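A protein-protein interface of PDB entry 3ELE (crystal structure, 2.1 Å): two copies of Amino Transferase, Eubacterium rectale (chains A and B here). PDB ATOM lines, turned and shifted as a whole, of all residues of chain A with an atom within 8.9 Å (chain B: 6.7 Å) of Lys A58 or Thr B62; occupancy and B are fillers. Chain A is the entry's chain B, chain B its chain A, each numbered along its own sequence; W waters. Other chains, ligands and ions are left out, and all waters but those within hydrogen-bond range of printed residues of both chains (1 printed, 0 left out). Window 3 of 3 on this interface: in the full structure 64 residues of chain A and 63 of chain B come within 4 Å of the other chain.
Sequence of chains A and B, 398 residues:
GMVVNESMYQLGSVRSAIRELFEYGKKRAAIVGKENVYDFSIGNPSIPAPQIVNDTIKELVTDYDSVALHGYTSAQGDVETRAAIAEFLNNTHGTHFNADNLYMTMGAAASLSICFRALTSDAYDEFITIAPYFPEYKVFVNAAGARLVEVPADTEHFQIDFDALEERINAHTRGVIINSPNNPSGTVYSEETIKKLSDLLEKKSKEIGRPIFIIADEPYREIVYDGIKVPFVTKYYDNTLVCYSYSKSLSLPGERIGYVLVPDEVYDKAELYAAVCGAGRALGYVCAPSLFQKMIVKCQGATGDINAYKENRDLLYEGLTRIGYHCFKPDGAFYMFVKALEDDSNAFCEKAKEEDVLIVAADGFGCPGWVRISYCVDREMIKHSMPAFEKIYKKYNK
The backbone carbonyl oxygen (O) of Val B61 sits at hydrogen-bond distance from the side-chain amide nitrogen (ND2) of Asn A54, 3.4 Å away.
The side-chain carboxylate (OD1) of Asp A55 lies within salt-bridge range of the side-chain amino group (NZ) of Lys A58 (3.5 Å). The backbone carbonyl oxygen (O) of Lys B58 sits at hydrogen-bond distance from the side-chain hydroxyl (OG1) of Thr B62 (2.7 Å). The backbone carbonyl oxygen of Lys A58 lies within hydrogen-bond range of the side-chain hydroxyl of Thr A62 (2.7 Å).
Among the printed residues, merely in contact across the chains: Ile A57 with Val B61 (3.6 Å), Ile A57 with Ile B57 (3.6 Å), Thr A62 with Lys B58 (3.7 Å), Lys A58 with Val B61 (3.7 Å), Val A61 with Ile B57 (3.7 Å), Val A61 with Lys B58 (3.7 Å) and Lys A58 with Thr B62 (3.8 Å).
Ile A52 touches none of the printed residues of chain B. Of the printed residues of chain B, Asn A54 touches Val B61 (3.1 Å). Lys A58 touches two residues of chain B. Leu A60 touches none of the printed residues of chain B. Printed residues of chain B within 4 Å of Val A61: Ile B57 and Lys B58. Printed residues of chain B within 4 Å of Thr A62: Lys B58 (3.7 Å). Printed residues of chain A within 4 Å of Lys B58: Val A61 (3.7 Å) and Thr A62 (3.7 Å). Thr B62 touches just one residue of chain A: Lys A58. No residue of chain A comes within 4 Å of Asp B63. The nearest residue of chain B that does not touch Lys A58 is Lys B58 (4.7 Å). The nearest residue of chain A that does not touch Thr B62 is Asn A54 (5.6 Å).
Of the 9 printed residues of chain B, 4 touch a printed residue of chain A. Hydrophobic or aromatic side chains of chain B that line the printed part of chain A: Ile B57 and Val B61. Printed residues of chain A that touch a printed residue of chain B: Asn A54, Ile A57, Lys A58, Val A61 and Thr A62. Hydrophobic or aromatic side chains of chain A within 4 Å of the printed part of chain B: Ile A57 and Val A61. Among the printed residues, 8 pairs touch across the chains. Among the printed residues, no Asp or Glu carboxylate lies within 4 Å of a Lys or Arg side-chain nitrogen of the other chain.
Ile A57 touches its own counterpart, Ile B57. Ile A57 touches Val B61, and with the chains exchanged Val A61 touches Ile B57. Lys A58 touches Val B61, and with the chains exchanged Val A61 touches Lys B58. Lys A58 touches Thr B62, and with the chains exchanged Thr A62 touches Lys B58. 9 positions are printed for both chains. Of the 8 pairs that touch across the chains among the printed residues, 7 have their exchanged pair printed and touching as well.
Water W1 lies within hydrogen-bond range of the backbone carbonyl oxygen of Tyr B64 (2.6 Å), the backbone carbonyl oxygen of Val B61 (2.8 Å) and the side-chain amide nitrogen of Asn A54 (3.1 Å).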
ATOM      1  N   GLN A  51      -6.148  -2.436  12.271  1.00  0.00           N
ATOM      2  CA  GLN A  51      -6.571  -3.710  11.669  1.00  0.00           C
ATOM      3  C   GLN A  51      -6.305  -4.965  12.538  1.00  0.00           C
ATOM      4  O   GLN A  51      -7.033  -5.949  12.399  1.00  0.00           O
ATOM      5  CB  GLN A  51      -6.003  -3.870  10.234  1.00  0.00           C
ATOM      6  CG  GLN A  51      -6.626  -5.006   9.386  1.00  0.00           C
ATOM      7  CD  GLN A  51      -8.133  -4.840   9.104  1.00  0.00           C
ATOM      8  OE1 GLN A  51      -8.608  -3.734   8.845  1.00  0.00           O
ATOM      9  NE2 GLN A  51      -8.878  -5.953   9.125  1.00  0.00           N
ATOM     10  N   ILE A  52      -5.317  -4.907  13.445  1.00  0.00           N
ATOM     11  CA  ILE A  52      -4.979  -6.027  14.353  1.00  0.00           C
ATOM     12  C   ILE A  52      -6.172  -6.488  15.196  1.00  0.00           C
ATOM     13  O   ILE A  52      -6.300  -7.680  15.454  1.00  0.00           O
ATOM     14  CB  ILE A  52      -3.723  -5.710  15.276  1.00  0.00           C
ATOM     15  CG1 ILE A  52      -3.219  -6.941  16.069  1.00  0.00           C
ATOM     16  CG2 ILE A  52      -4.024  -4.576  16.260  1.00  0.00           C
ATOM     17  CD1 ILE A  52      -2.803  -8.165  15.259  1.00  0.00           C
ATOM     18  N   VAL A  53      -7.041  -5.544  15.576  1.00  0.00           N
ATOM     19  CA  VAL A  53      -8.246  -5.815  16.362  1.00  0.00           C
ATOM     20  C   VAL A  53      -9.172  -6.789  15.646  1.00  0.00           C
ATOM     21  O   VAL A  53      -9.430  -7.881  16.162  1.00  0.00           O
ATOM     22  CB  VAL A  53      -9.018  -4.493  16.708  1.00  0.00           C
ATOM     23  CG1 VAL A  53     -10.411  -4.772  17.256  1.00  0.00           C
ATOM     24  CG2 VAL A  53      -8.213  -3.665  17.701  1.00  0.00           C
ATOM     25  N   ASN A  54      -9.650  -6.388  14.465  1.00  0.00           N
ATOM     26  CA  ASN A  54     -10.565  -7.216  13.669  1.00  0.00           C
ATOM     27  C   ASN A  54      -9.912  -8.523  13.230  1.00  0.00           C
ATOM     28  O   ASN A  54     -10.563  -9.573  13.264  1.00  0.00           O
ATOM     29  CB  ASN A  54     -11.166  -6.439  12.471  1.00  0.00           C
ATOM     30  CG  ASN A  54     -12.305  -5.475  12.881  1.00  0.00           C
ATOM     31  OD1 ASN A  54     -12.839  -5.515  14.002  1.00  0.00           O
ATOM     32  ND2 ASN A  54     -12.693  -4.621  11.949  1.00  0.00           N
ATOM     33  N   ASP A  55      -8.631  -8.461  12.856  1.00  0.00           N
ATOM     34  CA  ASP A  55      -7.869  -9.668  12.508  1.00  0.00           C
ATOM     35  C   ASP A  55      -7.817 -10.668  13.674  1.00  0.00           C
ATOM     36  O   ASP A  55      -8.093 -11.846  13.485  1.00  0.00           O
ATOM     37  CB  ASP A  55      -6.461  -9.321  12.014  1.00  0.00           C
ATOM     38  CG  ASP A  55      -6.462  -8.595  10.651  1.00  0.00           C
ATOM     39  OD1 ASP A  55      -7.550  -8.291  10.088  1.00  0.00           O
ATOM     40  OD2 ASP A  55      -5.350  -8.325  10.149  1.00  0.00           O
ATOM     41  N   THR A  56      -7.512 -10.184  14.873  1.00  0.00           N
ATOM     42  CA  THR A  56      -7.488 -11.041  16.072  1.00  0.00           C
ATOM     43  C   THR A  56      -8.878 -11.647  16.383  1.00  0.00           C
ATOM     44  O   THR A  56      -8.951 -12.824  16.733  1.00  0.00           O
ATOM     45  CB  THR A  56      -6.883 -10.311  17.305  1.00  0.00           C
ATOM     46  OG1 THR A  56      -5.566  -9.844  16.972  1.00  0.00           O
ATOM     47  CG2 THR A  56      -6.788 -11.262  18.524  1.00  0.00           C
ATOM     48  N   ILE A  57      -9.958 -10.872  16.215  1.00  0.00           N
ATOM     49  CA  ILE A  57     -11.328 -11.378  16.452  1.00  0.00           C
ATOM     50  C   ILE A  57     -11.650 -12.532  15.460  1.00  0.00           C
ATOM     51  O   ILE A  57     -12.186 -13.557  15.880  1.00  0.00           O
ATOM     52  CB  ILE A  57     -12.398 -10.255  16.409  1.00  0.00           C
ATOM     53  CG1 ILE A  57     -12.193  -9.253  17.552  1.00  0.00           C
ATOM     54  CG2 ILE A  57     -13.818 -10.834  16.549  1.00  0.00           C
ATOM     55  CD1 ILE A  57     -12.991  -7.977  17.395  1.00  0.00           C
ATOM     56  N   LYS A  58     -11.302 -12.363  14.176  1.00  0.00           N
ATOM     57  CA  LYS A  58     -11.450 -13.439  13.163  1.00  0.00           C
ATOM     58  C   LYS A  58     -10.663 -14.682  13.592  1.00  0.00           C
ATOM     59  O   LYS A  58     -11.226 -15.778  13.600  1.00  0.00           O
ATOM     60  CB  LYS A  58     -10.984 -13.015  11.754  1.00  0.00           C
ATOM     61  CG  LYS A  58     -11.973 -12.163  10.985  1.00  0.00           C
ATOM     62  CD  LYS A  58     -11.451 -11.771   9.575  1.00  0.00           C
ATOM     63  CE  LYS A  58     -10.363 -10.679   9.642  1.00  0.00           C
ATOM     64  NZ  LYS A  58      -9.877 -10.217   8.322  1.00  0.00           N
ATOM     65  N   GLU A  59      -9.380 -14.483  13.943  1.00  0.00           N
ATOM     66  CA  GLU A  59      -8.494 -15.559  14.456  1.00  0.00           C
ATOM     67  C   GLU A  59      -9.042 -16.329  15.654  1.00  0.00           C
ATOM     68  O   GLU A  59      -8.994 -17.557  15.653  1.00  0.00           O
ATOM     69  CB  GLU A  59      -7.129 -15.025  14.906  1.00  0.00           C
ATOM     70  CG  GLU A  59      -6.060 -14.968  13.872  1.00  0.00           C
ATOM     71  CD  GLU A  59      -4.678 -14.718  14.503  1.00  0.00           C
ATOM     72  OE1 GLU A  59      -4.603 -13.963  15.521  1.00  0.00           O
ATOM     73  OE2 GLU A  59      -3.675 -15.286  13.974  1.00  0.00           O
ATOM     74  N   LEU A  60      -9.498 -15.599  16.675  1.00  0.00           N
ATOM     75  CA  LEU A  60     -10.035 -16.208  17.911  1.00  0.00           C
ATOM     76  C   LEU A  60     -11.300 -17.030  17.624  1.00  0.00           C
ATOM     77  O   LEU A  60     -11.413 -18.173  18.070  1.00  0.00           O
ATOM     78  CB  LEU A  60     -10.288 -15.155  19.004  1.00  0.00           C
ATOM     79  CG  LEU A  60      -9.045 -14.538  19.658  1.00  0.00           C
ATOM     80  CD1 LEU A  60      -9.380 -13.313  20.475  1.00  0.00           C
ATOM     81  CD2 LEU A  60      -8.328 -15.570  20.513  1.00  0.00           C
ATOM     82  N   VAL A  61     -12.217 -16.453  16.852  1.00  0.00           N
ATOM     83  CA  VAL A  61     -13.456 -17.132  16.436  1.00  0.00           C
ATOM     84  C   VAL A  61     -13.203 -18.348  15.502  1.00  0.00           C
ATOM     85  O   VAL A  61     -13.897 -19.368  15.597  1.00  0.00           O
ATOM     86  CB  VAL A  61     -14.463 -16.077  15.856  1.00  0.00           C
ATOM     87  CG1 VAL A  61     -15.497 -16.685  14.982  1.00  0.00           C
ATOM     88  CG2 VAL A  61     -15.104 -15.258  17.032  1.00  0.00           C
ATOM     89  N   THR A  62     -12.198 -18.254  14.634  1.00  0.00           N
ATOM     90  CA  THR A  62     -11.847 -19.346  13.730  1.00  0.00           C
ATOM     91  C   THR A  62     -11.045 -20.461  14.429  1.00  0.00           C
ATOM     92  O   THR A  62     -11.364 -21.648  14.264  1.00  0.00           O
ATOM     93  CB  THR A  62     -11.025 -18.837  12.509  1.00  0.00           C
ATOM     94  OG1 THR A  62     -11.741 -17.793  11.836  1.00  0.00           O
ATOM     95  CG2 THR A  62     -10.739 -19.979  11.524  1.00  0.00           C
ATOM     96  N   ASP A  63     -10.033 -20.075  15.216  1.00  0.00           N
ATOM     97  CA  ASP A  63      -9.062 -21.037  15.791  1.00  0.00           C
ATOM     98  C   ASP A  63      -9.211 -21.459  17.246  1.00  0.00           C
ATOM     99  O   ASP A  63      -8.911 -22.604  17.575  1.00  0.00           O
ATOM    100  CB  ASP A  63      -7.630 -20.507  15.571  1.00  0.00           C
ATOM    101  CG  ASP A  63      -7.322 -20.218  14.099  1.00  0.00           C
ATOM    102  OD1 ASP A  63      -7.952 -20.829  13.207  1.00  0.00           O
ATOM    103  OD2 ASP A  63      -6.444 -19.368  13.837  1.00  0.00           O
ATOM    104  N   TYR A  64      -9.650 -20.556  18.113  1.00  0.00           N
ATOM    105  CA  TYR A  64      -9.768 -20.861  19.545  1.00  0.00           C
ATOM    106  C   TYR A  64     -11.008 -21.758  19.767  1.00  0.00           C
ATOM    107  O   TYR A  64     -12.026 -21.600  19.068  1.00  0.00           O
ATOM    108  CB  TYR A  64      -9.893 -19.550  20.342  1.00  0.00           C
ATOM    109  CG  TYR A  64      -9.424 -19.552  21.782  1.00  0.00           C
ATOM    110  CD1 TYR A  64     -10.181 -20.169  22.803  1.00  0.00           C
ATOM    111  CD2 TYR A  64      -8.266 -18.839  22.155  1.00  0.00           C
ATOM    112  CE1 TYR A  64      -9.761 -20.121  24.157  1.00  0.00           C
ATOM    113  CE2 TYR A  64      -7.837 -18.786  23.491  1.00  0.00           C
ATOM    114  CZ  TYR A  64      -8.582 -19.428  24.487  1.00  0.00           C
ATOM    115  OH  TYR A  64      -8.131 -19.342  25.787  1.00  0.00           O
ATOM    116  N   LEU A  69     -13.421 -20.101  24.417  1.00  0.00           N
ATOM    117  CA  LEU A  69     -13.403 -18.723  23.898  1.00  0.00           C
ATOM    118  C   LEU A  69     -14.523 -17.839  24.485  1.00  0.00           C
ATOM    119  O   LEU A  69     -14.270 -16.677  24.858  1.00  0.00           O
ATOM    120  CB  LEU A  69     -13.514 -18.707  22.354  1.00  0.00           C
ATOM    121  CG  LEU A  69     -13.618 -17.327  21.665  1.00  0.00           C
ATOM    122  CD1 LEU A  69     -12.461 -16.432  22.087  1.00  0.00           C
ATOM    123  CD2 LEU A  69     -13.663 -17.498  20.149  1.00  0.00           C
ATOM    124  N   LEU A 291     -14.059 -12.635  24.679  1.00  0.00           N
ATOM    125  CA  LEU A 291     -13.451 -12.428  23.337  1.00  0.00           C
ATOM    126  C   LEU A 291     -12.467 -11.256  23.302  1.00  0.00           C
ATOM    127  O   LEU A 291     -11.395 -11.366  22.716  1.00  0.00           O
ATOM    128  CB  LEU A 291     -14.539 -12.168  22.275  1.00  0.00           C
ATOM    129  CG  LEU A 291     -14.086 -11.941  20.816  1.00  0.00           C
ATOM    130  CD1 LEU A 291     -13.289 -13.129  20.331  1.00  0.00           C
ATOM    131  CD2 LEU A 291     -15.282 -11.674  19.921  1.00  0.00           C
ATOM    132  N   MET A 295      -8.504 -10.970  22.901  1.00  0.00           N
ATOM    133  CA  MET A 295      -8.008 -10.095  21.819  1.00  0.00           C
ATOM    134  C   MET A 295      -6.917  -9.139  22.326  1.00  0.00           C
ATOM    135  O   MET A 295      -5.877  -9.002  21.686  1.00  0.00           O
ATOM    136  CB  MET A 295      -9.184  -9.338  21.146  1.00  0.00           C
ATOM    137  CG  MET A 295      -8.828  -8.258  20.105  1.00  0.00           C
ATOM    138  SD  MET A 295      -8.497  -6.484  20.867  1.00  0.00           S
ATOM    139  CE  MET A 295     -10.284  -6.021  21.389  1.00  0.00           C
ATOM    140  N   ILE B  57     -20.154 -13.289  13.844  1.00  0.00           N
ATOM    141  CA  ILE B  57     -19.035 -12.466  14.358  1.00  0.00           C
ATOM    142  C   ILE B  57     -18.005 -12.219  13.239  1.00  0.00           C
ATOM    143  O   ILE B  57     -17.553 -11.079  13.044  1.00  0.00           O
ATOM    144  CB  ILE B  57     -18.343 -13.102  15.589  1.00  0.00           C
ATOM    145  CG1 ILE B  57     -19.253 -13.088  16.814  1.00  0.00           C
ATOM    146  CG2 ILE B  57     -17.064 -12.340  15.962  1.00  0.00           C
ATOM    147  CD1 ILE B  57     -18.732 -13.937  17.956  1.00  0.00           C
ATOM    148  N   LYS B  58     -17.646 -13.285  12.517  1.00  0.00           N
ATOM    149  CA  LYS B  58     -16.735 -13.187  11.366  1.00  0.00           C
ATOM    150  C   LYS B  58     -17.245 -12.208  10.295  1.00  0.00           C
ATOM    151  O   LYS B  58     -16.470 -11.394   9.790  1.00  0.00           O
ATOM    152  CB  LYS B  58     -16.456 -14.571  10.750  1.00  0.00           C
ATOM    153  CG  LYS B  58     -15.423 -15.382  11.538  1.00  0.00           C
ATOM    154  CD  LYS B  58     -15.139 -16.791  10.956  1.00  0.00           C
ATOM    155  CE  LYS B  58     -16.228 -17.820  11.334  1.00  0.00           C
ATOM    156  NZ  LYS B  58     -15.858 -19.233  11.004  1.00  0.00           N
ATOM    157  N   GLU B  59     -18.542 -12.278   9.987  1.00  0.00           N
ATOM    158  CA  GLU B  59     -19.178 -11.396   8.987  1.00  0.00           C
ATOM    159  C   GLU B  59     -19.172  -9.906   9.360  1.00  0.00           C
ATOM    160  O   GLU B  59     -18.921  -9.050   8.503  1.00  0.00           O
ATOM    161  CB  GLU B  59     -20.618 -11.842   8.706  1.00  0.00           C
ATOM    162  CG  GLU B  59     -20.719 -13.144   7.889  1.00  0.00           C
ATOM    163  CD  GLU B  59     -22.155 -13.684   7.798  1.00  0.00           C
ATOM    164  OE1 GLU B  59     -23.118 -12.908   8.054  1.00  0.00           O
ATOM    165  OE2 GLU B  59     -22.318 -14.883   7.453  1.00  0.00           O
ATOM    166  N   LEU B  60     -19.452  -9.607  10.629  1.00  0.00           N
ATOM    167  CA  LEU B  60     -19.482  -8.225  11.105  1.00  0.00           C
ATOM    168  C   LEU B  60     -18.080  -7.604  11.065  1.00  0.00           C
ATOM    169  O   LEU B  60     -17.892  -6.510  10.548  1.00  0.00           O
ATOM    170  CB  LEU B  60     -20.094  -8.151  12.510  1.00  0.00           C
ATOM    171  CG  LEU B  60     -21.563  -8.590  12.569  1.00  0.00           C
ATOM    172  CD1 LEU B  60     -22.013  -8.617  14.009  1.00  0.00           C
ATOM    173  CD2 LEU B  60     -22.482  -7.719  11.701  1.00  0.00           C
ATOM    174  N   VAL B  61     -17.111  -8.342  11.594  1.00  0.00           N
ATOM    175  CA  VAL B  61     -15.698  -7.957  11.579  1.00  0.00           C
ATOM    176  C   VAL B  61     -15.165  -7.744  10.139  1.00  0.00           C
ATOM    177  O   VAL B  61     -14.357  -6.839   9.912  1.00  0.00           O
ATOM    178  CB  VAL B  61     -14.847  -8.987  12.403  1.00  0.00           C
ATOM    179  CG1 VAL B  61     -13.396  -8.951  12.042  1.00  0.00           C
ATOM    180  CG2 VAL B  61     -15.061  -8.758  13.921  1.00  0.00           C
ATOM    181  N   THR B  62     -15.671  -8.515   9.177  1.00  0.00           N
ATOM    182  CA  THR B  62     -15.233  -8.420   7.772  1.00  0.00           C
ATOM    183  C   THR B  62     -15.969  -7.357   6.933  1.00  0.00           C
ATOM    184  O   THR B  62     -15.323  -6.677   6.134  1.00  0.00           O
ATOM    185  CB  THR B  62     -15.366  -9.799   7.062  1.00  0.00           C
ATOM    186  OG1 THR B  62     -14.704 -10.793   7.842  1.00  0.00           O
ATOM    187  CG2 THR B  62     -14.743  -9.781   5.667  1.00  0.00           C
ATOM    188  N   ASP B  63     -17.291  -7.208   7.127  1.00  0.00           N
ATOM    189  CA  ASP B  63     -18.148  -6.340   6.278  1.00  0.00           C
ATOM    190  C   ASP B  63     -18.839  -5.124   6.899  1.00  0.00           C
ATOM    191  O   ASP B  63     -19.238  -4.223   6.167  1.00  0.00           O
ATOM    192  CB  ASP B  63     -19.243  -7.210   5.643  1.00  0.00           C
ATOM    193  CG  ASP B  63     -18.685  -8.378   4.829  1.00  0.00           C
ATOM    194  OD1 ASP B  63     -17.579  -8.272   4.247  1.00  0.00           O
ATOM    195  OD2 ASP B  63     -19.377  -9.411   4.765  1.00  0.00           O
ATOM    196  N   TYR B  64     -19.002  -5.087   8.214  1.00  0.00           N
ATOM    197  CA  TYR B  64     -19.681  -3.957   8.871  1.00  0.00           C
ATOM    198  C   TYR B  64     -18.630  -2.850   9.059  1.00  0.00           C
ATOM    199  O   TYR B  64     -17.497  -3.156   9.440  1.00  0.00           O
ATOM    200  CB  TYR B  64     -20.263  -4.406  10.223  1.00  0.00           C
ATOM    201  CG  TYR B  64     -21.426  -3.589  10.749  1.00  0.00           C
ATOM    202  CD1 TYR B  64     -21.221  -2.364  11.383  1.00  0.00           C
ATOM    203  CD2 TYR B  64     -22.741  -4.063  10.645  1.00  0.00           C
ATOM    204  CE1 TYR B  64     -22.299  -1.610  11.889  1.00  0.00           C
ATOM    205  CE2 TYR B  64     -23.828  -3.331  11.150  1.00  0.00           C
ATOM    206  CZ  TYR B  64     -23.602  -2.103  11.767  1.00  0.00           C
ATOM    207  OH  TYR B  64     -24.676  -1.387  12.264  1.00  0.00           O
ATOM    208  N   LEU B  69     -19.446  -0.524  13.803  1.00  0.00           N
ATOM    209  CA  LEU B  69     -19.432  -1.828  14.506  1.00  0.00           C
ATOM    210  C   LEU B  69     -18.991  -1.694  15.970  1.00  0.00           C
ATOM    211  O   LEU B  69     -19.698  -2.122  16.889  1.00  0.00           O
ATOM    212  CB  LEU B  69     -18.489  -2.821  13.799  1.00  0.00           C
ATOM    213  CG  LEU B  69     -18.341  -4.250  14.348  1.00  0.00           C
ATOM    214  CD1 LEU B  69     -19.687  -4.955  14.506  1.00  0.00           C
ATOM    215  CD2 LEU B  69     -17.401  -5.057  13.453  1.00  0.00           C
HETATM  216  O   HOH W   1     -15.244  -4.190  10.325  1.00  0.00           O
